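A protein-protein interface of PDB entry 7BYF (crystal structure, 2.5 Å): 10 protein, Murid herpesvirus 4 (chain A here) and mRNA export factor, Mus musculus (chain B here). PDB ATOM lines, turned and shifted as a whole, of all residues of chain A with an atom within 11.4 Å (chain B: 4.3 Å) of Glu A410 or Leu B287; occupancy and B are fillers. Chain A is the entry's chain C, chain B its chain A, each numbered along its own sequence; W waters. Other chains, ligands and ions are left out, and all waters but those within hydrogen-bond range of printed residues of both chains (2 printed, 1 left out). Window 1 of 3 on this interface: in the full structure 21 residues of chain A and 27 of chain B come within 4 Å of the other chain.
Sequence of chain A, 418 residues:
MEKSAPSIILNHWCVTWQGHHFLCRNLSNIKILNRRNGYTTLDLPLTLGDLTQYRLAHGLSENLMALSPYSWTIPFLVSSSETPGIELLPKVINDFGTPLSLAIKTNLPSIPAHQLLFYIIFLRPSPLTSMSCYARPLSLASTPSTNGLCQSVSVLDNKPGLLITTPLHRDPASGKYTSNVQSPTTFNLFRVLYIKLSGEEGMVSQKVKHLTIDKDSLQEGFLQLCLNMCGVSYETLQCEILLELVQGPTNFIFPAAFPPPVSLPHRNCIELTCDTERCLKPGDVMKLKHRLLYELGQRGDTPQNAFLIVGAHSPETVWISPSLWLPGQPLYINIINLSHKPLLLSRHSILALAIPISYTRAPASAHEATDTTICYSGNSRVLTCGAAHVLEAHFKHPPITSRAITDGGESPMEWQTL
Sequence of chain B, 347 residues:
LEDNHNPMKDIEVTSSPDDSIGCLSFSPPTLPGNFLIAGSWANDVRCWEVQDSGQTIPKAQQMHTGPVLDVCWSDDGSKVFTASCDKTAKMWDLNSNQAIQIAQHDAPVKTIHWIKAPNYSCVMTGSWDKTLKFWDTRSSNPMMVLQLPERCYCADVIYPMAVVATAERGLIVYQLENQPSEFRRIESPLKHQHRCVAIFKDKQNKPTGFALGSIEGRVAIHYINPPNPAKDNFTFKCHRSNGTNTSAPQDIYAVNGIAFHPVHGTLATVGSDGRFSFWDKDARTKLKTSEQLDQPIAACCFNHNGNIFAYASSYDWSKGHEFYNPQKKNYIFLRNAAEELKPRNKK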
ATOM      1  N   ARG A 403      10.314 -41.889  -3.688  1.00  0.00           N
ATOM      2  CA  ARG A 403      10.316 -41.570  -5.141  1.00  0.00           C
ATOM      3  C   ARG A 403      11.712 -41.091  -5.553  1.00  0.00           C
ATOM      4  O   ARG A 403      12.488 -40.695  -4.661  1.00  0.00           O
ATOM      5  CB  ARG A 403       9.257 -40.509  -5.454  1.00  0.00           C
ATOM      6  CG  ARG A 403       9.808 -39.095  -5.570  1.00  0.00           C
ATOM      7  CD  ARG A 403       8.914 -38.191  -6.398  1.00  0.00           C
ATOM      8  NE  ARG A 403       8.782 -36.861  -5.819  1.00  0.00           N
ATOM      9  CZ  ARG A 403       9.802 -36.085  -5.473  1.00  0.00           C
ATOM     10  NH1 ARG A 403       9.578 -34.890  -4.954  1.00  0.00           N
ATOM     11  NH2 ARG A 403      11.042 -36.505  -5.650  1.00  0.00           N
ATOM     12  N   ILE A 405      14.125 -38.381  -7.323  1.00  0.00           N
ATOM     13  CA  ILE A 405      14.203 -36.926  -7.625  1.00  0.00           C
ATOM     14  C   ILE A 405      15.033 -36.691  -8.880  1.00  0.00           C
ATOM     15  O   ILE A 405      16.143 -37.144  -8.932  1.00  0.00           O
ATOM     16  CB  ILE A 405      14.807 -36.192  -6.427  1.00  0.00           C
ATOM     17  CG1 ILE A 405      14.056 -36.535  -5.152  1.00  0.00           C
ATOM     18  CG2 ILE A 405      14.855 -34.705  -6.676  1.00  0.00           C
ATOM     19  CD1 ILE A 405      14.737 -36.058  -3.938  1.00  0.00           C
ATOM     20  N   THR A 406      14.527 -35.877  -9.788  1.00  0.00           N
ATOM     21  CA  THR A 406      15.198 -35.681 -11.083  1.00  0.00           C
ATOM     22  C   THR A 406      15.848 -34.309 -11.243  1.00  0.00           C
ATOM     23  O   THR A 406      17.005 -34.264 -11.705  1.00  0.00           O
ATOM     24  CB  THR A 406      14.179 -35.893 -12.197  1.00  0.00           C
ATOM     25  OG1 THR A 406      13.415 -34.695 -12.181  1.00  0.00           O
ATOM     26  CG2 THR A 406      13.296 -37.091 -11.950  1.00  0.00           C
ATOM     27  N   ASP A 407      15.127 -33.232 -10.966  1.00  0.00           N
ATOM     28  CA  ASP A 407      15.699 -31.866 -11.174  1.00  0.00           C
ATOM     29  C   ASP A 407      16.173 -31.718 -12.625  1.00  0.00           C
ATOM     30  O   ASP A 407      17.334 -31.471 -12.856  1.00  0.00           O
ATOM     31  CB  ASP A 407      16.725 -31.499 -10.094  1.00  0.00           C
ATOM     32  CG  ASP A 407      17.685 -30.369 -10.416  1.00  0.00           C
ATOM     33  OD1 ASP A 407      17.342 -29.506 -11.245  1.00  0.00           O
ATOM     34  OD2 ASP A 407      18.781 -30.367  -9.815  1.00  0.00           O
ATOM     35  N   GLY A 408      15.278 -31.879 -13.576  1.00  0.00           N
ATOM     36  CA  GLY A 408      15.737 -31.707 -14.957  1.00  0.00           C
ATOM     37  C   GLY A 408      16.000 -30.254 -15.309  1.00  0.00           C
ATOM     38  O   GLY A 408      17.173 -29.878 -15.415  1.00  0.00           O
ATOM     39  N   GLY A 409      14.950 -29.438 -15.454  1.00  0.00           N
ATOM     40  CA  GLY A 409      15.190 -28.072 -15.957  1.00  0.00           C
ATOM     41  C   GLY A 409      14.684 -26.948 -15.091  1.00  0.00           C
ATOM     42  O   GLY A 409      13.639 -27.109 -14.488  1.00  0.00           O
ATOM     43  N   GLU A 410      15.449 -25.853 -15.087  1.00  0.00           N
ATOM     44  CA  GLU A 410      15.162 -24.601 -14.365  1.00  0.00           C
ATOM     45  C   GLU A 410      15.260 -23.462 -15.373  1.00  0.00           C
ATOM     46  O   GLU A 410      16.290 -22.840 -15.438  1.00  0.00           O
ATOM     47  CB  GLU A 410      16.092 -24.413 -13.169  1.00  0.00           C
ATOM     48  CG  GLU A 410      15.999 -23.038 -12.531  1.00  0.00           C
ATOM     49  CD  GLU A 410      16.877 -22.775 -11.317  1.00  0.00           C
ATOM     50  OE1 GLU A 410      17.080 -21.611 -10.963  1.00  0.00           O
ATOM     51  OE2 GLU A 410      17.331 -23.735 -10.711  1.00  0.00           O
ATOM     52  N   SER A 411      14.199 -23.252 -16.141  1.00  0.00           N
ATOM     53  CA  SER A 411      14.048 -22.219 -17.151  1.00  0.00           C
ATOM     54  C   SER A 411      13.611 -20.909 -16.496  1.00  0.00           C
ATOM     55  O   SER A 411      13.054 -20.908 -15.399  1.00  0.00           O
ATOM     56  CB  SER A 411      13.041 -22.665 -18.211  1.00  0.00           C
ATOM     57  OG  SER A 411      11.759 -22.904 -17.657  1.00  0.00           O
ATOM     58  N   PRO A 412      13.863 -19.771 -17.136  1.00  0.00           N
ATOM     59  CA  PRO A 412      13.491 -18.496 -16.517  1.00  0.00           C
ATOM     60  C   PRO A 412      11.993 -18.254 -16.584  1.00  0.00           C
ATOM     61  O   PRO A 412      11.303 -18.720 -17.499  1.00  0.00           O
ATOM     62  CB  PRO A 412      14.244 -17.450 -17.357  1.00  0.00           C
ATOM     63  CG  PRO A 412      15.115 -18.214 -18.289  1.00  0.00           C
ATOM     64  CD  PRO A 412      14.500 -19.563 -18.445  1.00  0.00           C
ATOM     65  N   MET A 413      11.495 -17.499 -15.603  1.00  0.00           N
ATOM     66  CA  MET A 413      10.175 -16.894 -15.738  1.00  0.00           C
ATOM     67  C   MET A 413      10.126 -16.041 -17.000  1.00  0.00           C
ATOM     68  O   MET A 413      11.121 -15.418 -17.374  1.00  0.00           O
ATOM     69  CB  MET A 413       9.872 -16.006 -14.524  1.00  0.00           C
ATOM     70  CG  MET A 413       9.548 -16.742 -13.277  1.00  0.00           C
ATOM     71  SD  MET A 413       9.243 -15.546 -11.974  1.00  0.00           S
ATOM     72  CE  MET A 413       8.778 -16.629 -10.629  1.00  0.00           C
ATOM     73  N   GLU A 414       8.975 -15.990 -17.656  1.00  0.00           N
ATOM     74  CA  GLU A 414       8.768 -14.940 -18.638  1.00  0.00           C
ATOM     75  C   GLU A 414       7.932 -13.863 -17.952  1.00  0.00           C
ATOM     76  O   GLU A 414       6.719 -14.005 -17.759  1.00  0.00           O
ATOM     77  CB  GLU A 414       8.165 -15.466 -19.937  1.00  0.00           C
ATOM     78  CG  GLU A 414       6.838 -16.125 -19.868  1.00  0.00           C
ATOM     79  CD  GLU A 414       6.320 -16.418 -21.257  1.00  0.00           C
ATOM     80  OE1 GLU A 414       6.334 -17.608 -21.654  1.00  0.00           O
ATOM     81  OE2 GLU A 414       5.933 -15.448 -21.954  1.00  0.00           O
ATOM     82  N   THR B 266      10.723 -20.226  -1.777  1.00  0.00           N
ATOM     83  CA  THR B 266      10.211 -20.510  -3.109  1.00  0.00           C
ATOM     84  C   THR B 266       8.677 -20.663  -3.060  1.00  0.00           C
ATOM     85  O   THR B 266       8.066 -20.665  -1.986  1.00  0.00           O
ATOM     86  CB  THR B 266      10.900 -21.763  -3.643  1.00  0.00           C
ATOM     87  OG1 THR B 266      11.064 -22.703  -2.571  1.00  0.00           O
ATOM     88  CG2 THR B 266      12.274 -21.414  -4.182  1.00  0.00           C
ATOM     89  N   PHE B 278       6.524 -24.946  -9.573  1.00  0.00           N
ATOM     90  CA  PHE B 278       7.395 -24.434  -8.524  1.00  0.00           C
ATOM     91  C   PHE B 278       8.285 -23.337  -9.090  1.00  0.00           C
ATOM     92  O   PHE B 278       8.786 -23.456 -10.215  1.00  0.00           O
ATOM     93  CB  PHE B 278       8.257 -25.546  -7.949  1.00  0.00           C
ATOM     94  CG  PHE B 278       7.472 -26.646  -7.297  1.00  0.00           C
ATOM     95  CD1 PHE B 278       6.320 -26.364  -6.576  1.00  0.00           C
ATOM     96  CD2 PHE B 278       7.899 -27.974  -7.400  1.00  0.00           C
ATOM     97  CE1 PHE B 278       5.598 -27.378  -5.972  1.00  0.00           C
ATOM     98  CE2 PHE B 278       7.189 -28.997  -6.797  1.00  0.00           C
ATOM     99  CZ  PHE B 278       6.033 -28.701  -6.085  1.00  0.00           C
ATOM    100  N   TRP B 279       8.502 -22.277  -8.300  1.00  0.00           N
ATOM    101  CA  TRP B 279       9.143 -21.063  -8.788  1.00  0.00           C
ATOM    102  C   TRP B 279      10.155 -20.521  -7.783  1.00  0.00           C
ATOM    103  O   TRP B 279      10.171 -20.903  -6.608  1.00  0.00           O
ATOM    104  CB  TRP B 279       8.111 -19.984  -9.066  1.00  0.00           C
ATOM    105  CG  TRP B 279       6.953 -20.459  -9.853  1.00  0.00           C
ATOM    106  CD1 TRP B 279       5.831 -21.077  -9.373  1.00  0.00           C
ATOM    107  CD2 TRP B 279       6.779 -20.345 -11.264  1.00  0.00           C
ATOM    108  NE1 TRP B 279       4.967 -21.353 -10.404  1.00  0.00           N
ATOM    109  CE2 TRP B 279       5.523 -20.919 -11.579  1.00  0.00           C
ATOM    110  CE3 TRP B 279       7.558 -19.817 -12.295  1.00  0.00           C
ATOM    111  CZ2 TRP B 279       5.030 -20.983 -12.888  1.00  0.00           C
ATOM    112  CZ3 TRP B 279       7.064 -19.873 -13.597  1.00  0.00           C
ATOM    113  CH2 TRP B 279       5.806 -20.448 -13.877  1.00  0.00           C
ATOM    114  N   THR B 285      12.894 -17.643 -11.814  1.00  0.00           N
ATOM    115  CA  THR B 285      13.005 -18.862 -12.585  1.00  0.00           C
ATOM    116  C   THR B 285      11.863 -19.791 -12.222  1.00  0.00           C
ATOM    117  O   THR B 285      11.191 -19.621 -11.196  1.00  0.00           O
ATOM    118  CB  THR B 285      14.323 -19.571 -12.314  1.00  0.00           C
ATOM    119  OG1 THR B 285      14.377 -19.928 -10.926  1.00  0.00           O
ATOM    120  CG2 THR B 285      15.477 -18.653 -12.637  1.00  0.00           C
ATOM    121  N   LYS B 286      11.675 -20.786 -13.081  1.00  0.00           N
ATOM    122  CA  LYS B 286      10.737 -21.881 -12.883  1.00  0.00           C
ATOM    123  C   LYS B 286      11.533 -23.135 -12.533  1.00  0.00           C
ATOM    124  O   LYS B 286      12.497 -23.482 -13.225  1.00  0.00           O
ATOM    125  CB  LYS B 286       9.878 -22.094 -14.146  1.00  0.00           C
ATOM    126  CG  LYS B 286       8.747 -23.093 -13.960  1.00  0.00           C
ATOM    127  CD  LYS B 286       7.698 -23.086 -15.093  1.00  0.00           C
ATOM    128  CE  LYS B 286       8.187 -23.808 -16.322  1.00  0.00           C
ATOM    129  NZ  LYS B 286       8.971 -25.002 -15.918  1.00  0.00           N
ATOM    130  N   LEU B 287      11.147 -23.798 -11.450  1.00  0.00           N
ATOM    131  CA  LEU B 287      11.900 -24.955 -10.983  1.00  0.00           C
ATOM    132  C   LEU B 287      11.336 -26.268 -11.515  1.00  0.00           C
ATOM    133  O   LEU B 287      12.095 -27.196 -11.817  1.00  0.00           O
ATOM    134  CB  LEU B 287      11.916 -24.991  -9.452  1.00  0.00           C
ATOM    135  CG  LEU B 287      12.318 -23.738  -8.694  1.00  0.00           C
ATOM    136  CD1 LEU B 287      12.202 -24.003  -7.214  1.00  0.00           C
ATOM    137  CD2 LEU B 287      13.723 -23.337  -9.058  1.00  0.00           C
ATOM    138  N   LYS B 288      10.015 -26.363 -11.626  1.00  0.00           N
ATOM    139  CA  LYS B 288       9.366 -27.582 -12.069  1.00  0.00           C
ATOM    140  C   LYS B 288       7.974 -27.217 -12.568  1.00  0.00           C
ATOM    141  O   LYS B 288       7.376 -26.240 -12.115  1.00  0.00           O
ATOM    142  CB  LYS B 288       9.298 -28.622 -10.943  1.00  0.00           C
ATOM    143  CG  LYS B 288       8.723 -29.978 -11.361  1.00  0.00           C
ATOM    144  CD  LYS B 288       8.806 -31.033 -10.257  1.00  0.00           C
ATOM    145  CE  LYS B 288       9.971 -31.995 -10.476  1.00  0.00           C
ATOM    146  NZ  LYS B 288       9.771 -32.949 -11.620  1.00  0.00           N
ATOM    147  N   GLU B 340      13.027 -30.434  -3.849  1.00  0.00           N
ATOM    148  CA  GLU B 340      12.700 -29.697  -5.088  1.00  0.00           C
ATOM    149  C   GLU B 340      12.362 -28.237  -4.861  1.00  0.00           C
ATOM    150  O   GLU B 340      12.397 -27.534  -5.811  1.00  0.00           O
ATOM    151  CB  GLU B 340      11.513 -30.294  -5.808  1.00  0.00           C
ATOM    152  CG  GLU B 340      11.147 -31.649  -5.306  1.00  0.00           C
ATOM    153  CD  GLU B 340      10.357 -32.459  -6.304  1.00  0.00           C
ATOM    154  OE1 GLU B 340       9.153 -32.511  -6.202  1.00  0.00           O
ATOM    155  OE2 GLU B 340      10.974 -33.039  -7.153  1.00  0.00           O
ATOM    156  N   ARG B 344      18.387 -22.979  -6.526  1.00  0.00           N
ATOM    157  CA  ARG B 344      19.631 -23.459  -7.185  1.00  0.00           C
ATOM    158  C   ARG B 344      20.712 -22.376  -7.075  1.00  0.00           C
ATOM    159  O   ARG B 344      20.331 -21.216  -6.820  1.00  0.00           O
ATOM    160  CB  ARG B 344      19.356 -23.814  -8.649  1.00  0.00           C
ATOM    161  CG  ARG B 344      20.165 -24.996  -9.166  1.00  0.00           C
ATOM    162  CD  ARG B 344      21.558 -24.592  -9.609  1.00  0.00           C
ATOM    163  NE  ARG B 344      21.581 -23.280 -10.241  1.00  0.00           N
ATOM    164  CZ  ARG B 344      22.676 -22.688 -10.703  1.00  0.00           C
ATOM    165  NH1 ARG B 344      22.596 -21.493 -11.264  1.00  0.00           N
ATOM    166  NH2 ARG B 344      23.846 -23.291 -10.605  1.00  0.00           N
HETATM  167  O   HOH W   1      12.297 -33.700  -9.209  1.00  0.00           O
HETATM  168  O   HOH W   2      12.530 -29.695 -12.500  1.00  0.00           O
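The side-chain hydroxyl (OG1) of Thr B285 sits at hydrogen-bond distance from the side-chain carboxylate (OE1) of Glu A410 (3.2 Å).
N of Lys B286 lies within hydrogen-bond range of O of Ser A411 (2.7 Å).
The side-chain carboxylate of Glu B340 lies within salt-bridge range of the guanidinium group of Arg A403 (2.7 Å).
O of Leu B287 sits close to O of Gly A409 (3.1 Å).
O of Lys B286 touches CA of Glu A410, at 3.1 Å.
Glu A410 touches Leu B287 (CD to CD2, 3.9 Å).
Glu A410 touches Arg B344 (OE2 to CB, 2.9 Å).
O of Ser A411 touches CA of Thr B285, 3.5 Å away.
CA of Pro A412 touches CA of Thr B285, 3.98 Å away.
Met A413 touches Trp B279.
Met A413 touches Thr B285.
O of Phe B278 sits at hydrogen-bond distance from N of Leu B287, 2.7 Å away.
Printed residues of chain B within 4 Å of Glu A410: Thr B285 (3.2 Å), Lys B286 (3.1 Å), Leu B287 (3.9 Å) and Arg B344 (2.9 Å).
Of chain A, only Gly A409 (3.1 Å) and Glu A410 (3.9 Å) come within 4 Å of Leu B287.
Trp B279 touches just one residue of chain A: Met A413.
Thr B285 touches just these residues of chain A: Glu A410 (3.2 Å), Ser A411 (3.5 Å), Pro A412 (3.98 Å) and Met A413 (3.6 Å).
Arg B344 touches just one residue of chain A: Glu A410.
Of the printed residues of chain B, Pro A412 touches Thr B285.
Of the printed residues of chain B, Met A413 touches Trp B279 and Thr B285.
Of the printed residues of chain B, Ser A411 touches Thr B285 and Lys B286.
The nearest printed residue of chain B that does not touch Glu A410 is Lys B288 (6.1 Å).
The nearest residue of chain A that does not touch Leu B287 is Ser A411 (5.3 Å).
The nearest printed residue of chain B that does not touch Met A413 is Lys B286 (4.1 Å).
Water W1 lies within hydrogen-bond range of the side-chain carboxylate (OE2) of Glu B340 (2.5 Å), the backbone NH (N) of Thr A406 (3.2 Å) and the backbone NH (N) of Asp A407 (3.4 Å).
Water W2 bridges O of Leu B287 and O of Gly A409.
Of the 9 printed residues of chain B, 6 touch a printed residue of chain A.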
